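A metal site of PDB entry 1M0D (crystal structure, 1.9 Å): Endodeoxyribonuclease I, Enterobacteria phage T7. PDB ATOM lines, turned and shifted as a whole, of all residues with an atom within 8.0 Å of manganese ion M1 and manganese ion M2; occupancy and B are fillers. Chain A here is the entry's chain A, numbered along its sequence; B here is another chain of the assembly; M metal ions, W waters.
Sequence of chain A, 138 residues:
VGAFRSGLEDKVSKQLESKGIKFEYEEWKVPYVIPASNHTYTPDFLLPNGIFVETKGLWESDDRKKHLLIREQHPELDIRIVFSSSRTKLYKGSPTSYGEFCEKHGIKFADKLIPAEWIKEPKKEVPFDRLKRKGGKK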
ATOM      1  N   TYR A  41      17.934   3.403  17.545  1.00  0.00           N
ATOM      2  CA  TYR A  41      18.172   4.839  17.363  1.00  0.00           C
ATOM      3  C   TYR A  41      16.799   5.516  17.375  1.00  0.00           C
ATOM      4  O   TYR A  41      15.888   5.074  16.674  1.00  0.00           O
ATOM      5  CB  TYR A  41      18.859   5.078  16.009  1.00  0.00           C
ATOM      6  CG  TYR A  41      18.731   6.496  15.481  1.00  0.00           C
ATOM      7  CD1 TYR A  41      19.113   7.593  16.259  1.00  0.00           C
ATOM      8  CD2 TYR A  41      18.241   6.728  14.200  1.00  0.00           C
ATOM      9  CE1 TYR A  41      18.989   8.916  15.759  1.00  0.00           C
ATOM     10  CE2 TYR A  41      18.125   8.029  13.691  1.00  0.00           C
ATOM     11  CZ  TYR A  41      18.483   9.109  14.469  1.00  0.00           C
ATOM     12  OH  TYR A  41      18.333  10.373  13.964  1.00  0.00           O
ATOM     13  N   THR A  42      16.673   6.582  18.158  1.00  0.00           N
ATOM     14  CA  THR A  42      15.428   7.325  18.284  1.00  0.00           C
ATOM     15  C   THR A  42      15.566   8.724  17.647  1.00  0.00           C
ATOM     16  O   THR A  42      16.066   9.654  18.273  1.00  0.00           O
ATOM     17  CB  THR A  42      15.041   7.471  19.779  1.00  0.00           C
ATOM     18  OG1 THR A  42      14.805   6.164  20.324  1.00  0.00           O
ATOM     19  CG2 THR A  42      13.788   8.334  19.946  1.00  0.00           C
ATOM     20  N   PRO A  43      15.121   8.870  16.388  1.00  0.00           N
ATOM     21  CA  PRO A  43      15.218  10.187  15.742  1.00  0.00           C
ATOM     22  C   PRO A  43      14.395  11.211  16.540  1.00  0.00           C
ATOM     23  O   PRO A  43      13.391  10.857  17.144  1.00  0.00           O
ATOM     24  CB  PRO A  43      14.631   9.948  14.358  1.00  0.00           C
ATOM     25  CG  PRO A  43      14.776   8.473  14.129  1.00  0.00           C
ATOM     26  CD  PRO A  43      14.512   7.880  15.486  1.00  0.00           C
ATOM     27  N   ASP A  44      14.828  12.448  16.535  1.00  0.00           N
ATOM     28  CA  ASP A  44      14.132  13.488  17.286  1.00  0.00           C
ATOM     29  C   ASP A  44      12.668  13.729  16.907  1.00  0.00           C
ATOM     30  O   ASP A  44      11.765  13.580  17.739  1.00  0.00           O
ATOM     31  CB  ASP A  44      14.927  14.779  17.174  1.00  0.00           C
ATOM     32  CG  ASP A  44      16.258  14.662  17.871  1.00  0.00           C
ATOM     33  OD1 ASP A  44      16.236  14.280  19.056  1.00  0.00           O
ATOM     34  OD2 ASP A  44      17.306  14.942  17.270  1.00  0.00           O
ATOM     35  N   PHE A  45      12.434  14.092  15.655  1.00  0.00           N
ATOM     36  CA  PHE A  45      11.080  14.400  15.203  1.00  0.00           C
ATOM     37  C   PHE A  45      10.566  13.532  14.066  1.00  0.00           C
ATOM     38  O   PHE A  45      11.336  13.092  13.215  1.00  0.00           O
ATOM     39  CB  PHE A  45      10.990  15.860  14.733  1.00  0.00           C
ATOM     40  CG  PHE A  45      11.423  16.863  15.758  1.00  0.00           C
ATOM     41  CD1 PHE A  45      12.754  17.265  15.849  1.00  0.00           C
ATOM     42  CD2 PHE A  45      10.490  17.430  16.630  1.00  0.00           C
ATOM     43  CE1 PHE A  45      13.152  18.222  16.775  1.00  0.00           C
ATOM     44  CE2 PHE A  45      10.879  18.384  17.565  1.00  0.00           C
ATOM     45  CZ  PHE A  45      12.211  18.778  17.645  1.00  0.00           C
ATOM     46  N   VAL A  53      13.229  13.779  11.354  1.00  0.00           N
ATOM     47  CA  VAL A  53      14.249  14.811  11.400  1.00  0.00           C
ATOM     48  C   VAL A  53      15.045  14.705  12.688  1.00  0.00           C
ATOM     49  O   VAL A  53      14.491  14.731  13.777  1.00  0.00           O
ATOM     50  CB  VAL A  53      13.628  16.251  11.372  1.00  0.00           C
ATOM     51  CG1 VAL A  53      14.734  17.287  11.605  1.00  0.00           C
ATOM     52  CG2 VAL A  53      12.949  16.497  10.012  1.00  0.00           C
ATOM     53  N   GLU A  54      16.357  14.579  12.537  1.00  0.00           N
ATOM     54  CA  GLU A  54      17.266  14.514  13.682  1.00  0.00           C
ATOM     55  C   GLU A  54      17.871  15.919  13.829  1.00  0.00           C
ATOM     56  O   GLU A  54      18.439  16.434  12.871  1.00  0.00           O
ATOM     57  CB  GLU A  54      18.417  13.546  13.373  1.00  0.00           C
ATOM     58  CG  GLU A  54      19.588  13.574  14.386  1.00  0.00           C
ATOM     59  CD  GLU A  54      19.166  13.063  15.754  1.00  0.00           C
ATOM     60  OE1 GLU A  54      18.271  12.195  15.817  1.00  0.00           O
ATOM     61  OE2 GLU A  54      19.739  13.519  16.778  1.00  0.00           O
ATOM     62  N   THR A  55      17.721  16.558  14.980  1.00  0.00           N
ATOM     63  CA  THR A  55      18.376  17.852  15.170  1.00  0.00           C
ATOM     64  C   THR A  55      19.766  17.462  15.701  1.00  0.00           C
ATOM     65  O   THR A  55      19.908  16.508  16.465  1.00  0.00           O
ATOM     66  CB  THR A  55      17.617  18.755  16.166  1.00  0.00           C
ATOM     67  OG1 THR A  55      17.039  17.971  17.220  1.00  0.00           O
ATOM     68  CG2 THR A  55      16.502  19.482  15.391  1.00  0.00           C
ATOM     69  N   LYS A  56      20.794  18.200  15.296  1.00  0.00           N
ATOM     70  CA  LYS A  56      22.155  17.813  15.673  1.00  0.00           C
ATOM     71  C   LYS A  56      23.112  18.975  15.877  1.00  0.00           C
ATOM     72  O   LYS A  56      23.238  19.833  15.002  1.00  0.00           O
ATOM     73  CB  LYS A  56      22.729  16.907  14.576  1.00  0.00           C
ATOM     74  CG  LYS A  56      24.096  16.277  14.880  1.00  0.00           C
ATOM     75  CD  LYS A  56      23.992  15.324  16.077  1.00  0.00           C
ATOM     76  CE  LYS A  56      22.987  14.232  15.809  1.00  0.00           C
ATOM     77  NZ  LYS A  56      22.863  13.289  16.977  1.00  0.00           N
ATOM     78  N   GLY A  57      23.778  18.991  17.015  1.00  0.00           N
ATOM     79  CA  GLY A  57      24.797  19.999  17.260  1.00  0.00           C
ATOM     80  C   GLY A  57      26.081  19.292  16.861  1.00  0.00           C
ATOM     81  O   GLY A  57      26.427  19.217  15.683  1.00  0.00           O
ATOM     82  N   LEU A  58      26.773  18.727  17.845  1.00  0.00           N
ATOM     83  CA  LEU A  58      28.025  17.983  17.595  1.00  0.00           C
ATOM     84  C   LEU A  58      27.661  16.622  16.968  1.00  0.00           C
ATOM     85  O   LEU A  58      26.773  15.936  17.472  1.00  0.00           O
ATOM     86  CB  LEU A  58      28.751  17.753  18.926  1.00  0.00           C
ATOM     87  CG  LEU A  58      29.936  16.790  18.856  1.00  0.00           C
ATOM     88  CD1 LEU A  58      31.105  17.484  18.181  1.00  0.00           C
ATOM     89  CD2 LEU A  58      30.312  16.336  20.274  1.00  0.00           C
ATOM     90  N   ASP A  63      28.136   8.344  15.348  1.00  0.00           N
ATOM     91  CA  ASP A  63      26.806   8.839  14.976  1.00  0.00           C
ATOM     92  C   ASP A  63      26.679   8.862  13.447  1.00  0.00           C
ATOM     93  O   ASP A  63      25.636   8.487  12.892  1.00  0.00           O
ATOM     94  CB  ASP A  63      26.614  10.242  15.566  1.00  0.00           C
ATOM     95  CG  ASP A  63      25.156  10.621  15.690  1.00  0.00           C
ATOM     96  OD1 ASP A  63      24.349  10.172  14.863  1.00  0.00           O
ATOM     97  OD2 ASP A  63      24.814  11.384  16.631  1.00  0.00           O
ATOM     98  N   LYS A  66      26.353   5.353  12.233  1.00  0.00           N
ATOM     99  CA  LYS A  66      24.996   4.902  12.546  1.00  0.00           C
ATOM    100  C   LYS A  66      24.004   5.295  11.439  1.00  0.00           C
ATOM    101  O   LYS A  66      23.174   4.489  11.025  1.00  0.00           O
ATOM    102  CB  LYS A  66      24.541   5.514  13.867  1.00  0.00           C
ATOM    103  CG  LYS A  66      23.151   5.103  14.331  1.00  0.00           C
ATOM    104  CD  LYS A  66      22.760   5.864  15.588  1.00  0.00           C
ATOM    105  CE  LYS A  66      22.605   7.368  15.332  1.00  0.00           C
ATOM    106  NZ  LYS A  66      22.586   8.129  16.607  1.00  0.00           N
ATOM    107  N   HIS A  67      24.080   6.537  10.963  1.00  0.00           N
ATOM    108  CA  HIS A  67      23.175   6.958   9.899  1.00  0.00           C
ATOM    109  C   HIS A  67      23.375   6.179   8.605  1.00  0.00           C
ATOM    110  O   HIS A  67      22.410   5.853   7.902  1.00  0.00           O
ATOM    111  CB  HIS A  67      23.295   8.463   9.638  1.00  0.00           C
ATOM    112  CG  HIS A  67      22.455   9.276  10.577  1.00  0.00           C
ATOM    113  ND1 HIS A  67      22.830   9.535  11.880  1.00  0.00           N
ATOM    114  CD2 HIS A  67      21.202   9.764  10.444  1.00  0.00           C
ATOM    115  CE1 HIS A  67      21.838  10.140  12.511  1.00  0.00           C
ATOM    116  NE2 HIS A  67      20.837  10.289  11.662  1.00  0.00           N
ATOM    117  N   ILE A  81      18.674  15.471   8.549  1.00  0.00           N
ATOM    118  CA  ILE A  81      19.307  16.127   9.686  1.00  0.00           C
ATOM    119  C   ILE A  81      19.285  17.638   9.607  1.00  0.00           C
ATOM    120  O   ILE A  81      19.526  18.221   8.551  1.00  0.00           O
ATOM    121  CB  ILE A  81      20.797  15.668   9.803  1.00  0.00           C
ATOM    122  CG1 ILE A  81      20.865  14.144   9.921  1.00  0.00           C
ATOM    123  CG2 ILE A  81      21.465  16.321  11.022  1.00  0.00           C
ATOM    124  CD1 ILE A  81      22.287  13.564   9.853  1.00  0.00           C
ATOM    125  N   VAL A  82      18.931  18.276  10.722  1.00  0.00           N
ATOM    126  CA  VAL A  82      18.959  19.730  10.834  1.00  0.00           C
ATOM    127  C   VAL A  82      20.108  20.002  11.826  1.00  0.00           C
ATOM    128  O   VAL A  82      20.018  19.642  12.996  1.00  0.00           O
ATOM    129  CB  VAL A  82      17.641  20.314  11.382  1.00  0.00           C
ATOM    130  CG1 VAL A  82      17.858  21.783  11.812  1.00  0.00           C
ATOM    131  CG2 VAL A  82      16.541  20.234  10.289  1.00  0.00           C
ATOM    132  N   SER B   6      16.970  20.564  23.864  1.00  0.00           N
ATOM    133  CA  SER B   6      18.268  21.243  23.726  1.00  0.00           C
ATOM    134  C   SER B   6      17.838  22.559  23.083  1.00  0.00           C
ATOM    135  O   SER B   6      16.673  22.710  22.740  1.00  0.00           O
ATOM    136  CB  SER B   6      19.209  20.474  22.785  1.00  0.00           C
ATOM    137  OG  SER B   6      18.885  20.660  21.404  1.00  0.00           O
ATOM    138  N   LEU B   8      18.531  23.783  20.069  1.00  0.00           N
ATOM    139  CA  LEU B   8      18.114  23.504  18.700  1.00  0.00           C
ATOM    140  C   LEU B   8      16.779  22.753  18.685  1.00  0.00           C
ATOM    141  O   LEU B   8      15.902  23.029  17.856  1.00  0.00           O
ATOM    142  CB  LEU B   8      19.205  22.687  17.990  1.00  0.00           C
ATOM    143  CG  LEU B   8      18.996  22.333  16.516  1.00  0.00           C
ATOM    144  CD1 LEU B   8      18.817  23.603  15.683  1.00  0.00           C
ATOM    145  CD2 LEU B   8      20.214  21.538  16.035  1.00  0.00           C
ATOM    146  N   GLU B   9      16.615  21.797  19.583  1.00  0.00           N
ATOM    147  CA  GLU B   9      15.365  21.055  19.635  1.00  0.00           C
ATOM    148  C   GLU B   9      14.240  22.004  20.000  1.00  0.00           C
ATOM    149  O   GLU B   9      13.123  21.907  19.486  1.00  0.00           O
ATOM    150  CB  GLU B   9      15.442  19.927  20.663  1.00  0.00           C
ATOM    151  CG  GLU B   9      16.226  18.711  20.184  1.00  0.00           C
ATOM    152  CD  GLU B   9      16.288  17.630  21.254  1.00  0.00           C
ATOM    153  OE1 GLU B   9      15.338  17.543  22.064  1.00  0.00           O
ATOM    154  OE2 GLU B   9      17.275  16.877  21.270  1.00  0.00           O
ATOM    155  N   TYR B  25       7.591  13.541  18.910  1.00  0.00           N
ATOM    156  CA  TYR B  25       8.939  13.730  19.421  1.00  0.00           C
ATOM    157  C   TYR B  25       9.416  12.463  20.100  1.00  0.00           C
ATOM    158  O   TYR B  25       8.807  12.034  21.074  1.00  0.00           O
ATOM    159  CB  TYR B  25       8.951  14.881  20.422  1.00  0.00           C
ATOM    160  CG  TYR B  25      10.284  15.092  21.067  1.00  0.00           C
ATOM    161  CD1 TYR B  25      11.363  15.615  20.340  1.00  0.00           C
ATOM    162  CD2 TYR B  25      10.494  14.765  22.413  1.00  0.00           C
ATOM    163  CE1 TYR B  25      12.607  15.818  20.936  1.00  0.00           C
ATOM    164  CE2 TYR B  25      11.730  14.957  23.007  1.00  0.00           C
ATOM    165  CZ  TYR B  25      12.781  15.482  22.272  1.00  0.00           C
ATOM    166  OH  TYR B  25      14.012  15.654  22.853  1.00  0.00           O
ATOM    167  N   GLU B  26      10.505  11.881  19.599  1.00  0.00           N
ATOM    168  CA  GLU B  26      11.082  10.662  20.155  1.00  0.00           C
ATOM    169  C   GLU B  26      10.050   9.579  20.408  1.00  0.00           C
ATOM    170  O   GLU B  26      10.117   8.879  21.413  1.00  0.00           O
ATOM    171  CB  GLU B  26      11.799  10.961  21.467  1.00  0.00           C
ATOM    172  CG  GLU B  26      12.846  12.043  21.362  1.00  0.00           C
ATOM    173  CD  GLU B  26      13.676  12.150  22.629  1.00  0.00           C
ATOM    174  OE1 GLU B  26      13.091  12.134  23.734  1.00  0.00           O
ATOM    175  OE2 GLU B  26      14.918  12.265  22.522  1.00  0.00           O
HETATM  176 MN    MN M   1      19.273  15.083  18.053  1.00  0.00          MN
HETATM  177 MN    MN M   2      17.478  12.807  20.132  1.00  0.00          MN
HETATM  178  O   HOH W   1      16.637  14.017  21.761  1.00  0.00           O
HETATM  179  O   HOH W   2      16.166  11.191  20.688  1.00  0.00           O
HETATM  180  O   HOH W   3      18.962  13.804  19.773  1.00  0.00           O
HETATM  181  O   HOH W   4      19.254  12.014  21.636  1.00  0.00           O
HETATM  182  O   HOH W   5      21.511  15.182  18.910  1.00  0.00           O
HETATM  183  O   HOH W   6      18.656  16.994  19.075  1.00  0.00           O
HETATM  184  O   HOH W   7      18.087  11.452  18.465  1.00  0.00           O
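Residues that only touch manganese ion M2: Glu 26 of chain B (3.5 Å) and Thr 42 (3.9 Å). Of the 21 residues printed, 3 come within 4 Å of manganese ion M2. The nearest printed residue that does not touch manganese ion M2 is Glu 54 (4.1 Å).
OE2 of Glu 54 sits close to NZ of Lys 56. The backbone NH (N) of Val 82 sits at hydrogen-bond distance from the backbone carbonyl oxygen (O) of Glu 54, 2.9 Å away. The backbone carbonyl oxygen (O) of Asp 44 lies within hydrogen-bond range of the backbone NH (N) of Glu 26 of chain B. The side-chain carboxylate (OE1) of Glu 54 sits at hydrogen-bond distance from the side-chain hydroxyl (OH) of Tyr 41.
Water W3 is bound to manganese ion M2. Manganese ion M2 is bound by water W2, 2.2 Å away. Water W1 binds manganese ion M2. OD1 of Asp 44 is bound to manganese ion M2 (2.2 Å). Water W7 binds manganese ion M2 (2.2 Å). Water W4 is bound to manganese ion M2. Manganese ion M2 has six donor atoms within binding distance.
Manganese ion M1 is bound by OE2 of Glu 54 (2.1 Å), OD2 of Asp 44 (2.1 Å), water W3 (2.2 Å), O of Thr 55 (2.2 Å), water W6 (2.3 Å) and water W5 (2.4 Å). Manganese ion M1 has six donor atoms within binding distance.
Water W6 bridges the side-chain carboxylate (OE2) of Glu 9 of chain B (2.6 Å) and the side-chain hydroxyl (OG1) of Thr 55 (2.6 Å). Water W2 bridges OE2 of Glu 26 of chain B (2.5 Å) and O of Thr 42 (2.9 Å). Water W7 lies within hydrogen-bond range of O of Thr 42 (2.7 Å) and OE1 of Glu 54 (2.8 Å). Water W1 lies within hydrogen-bond range of the side-chain carboxylate of Glu 26 of chain B (2.6 Å), the side-chain carboxylate of Glu 9 of chain B (3.0 Å) and the side-chain hydroxyl of Tyr 25 of chain B (3.3 Å).
Three residues have an atom within 4 Å of manganese ion M1: Asp 44, Glu 54 and Thr 55.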
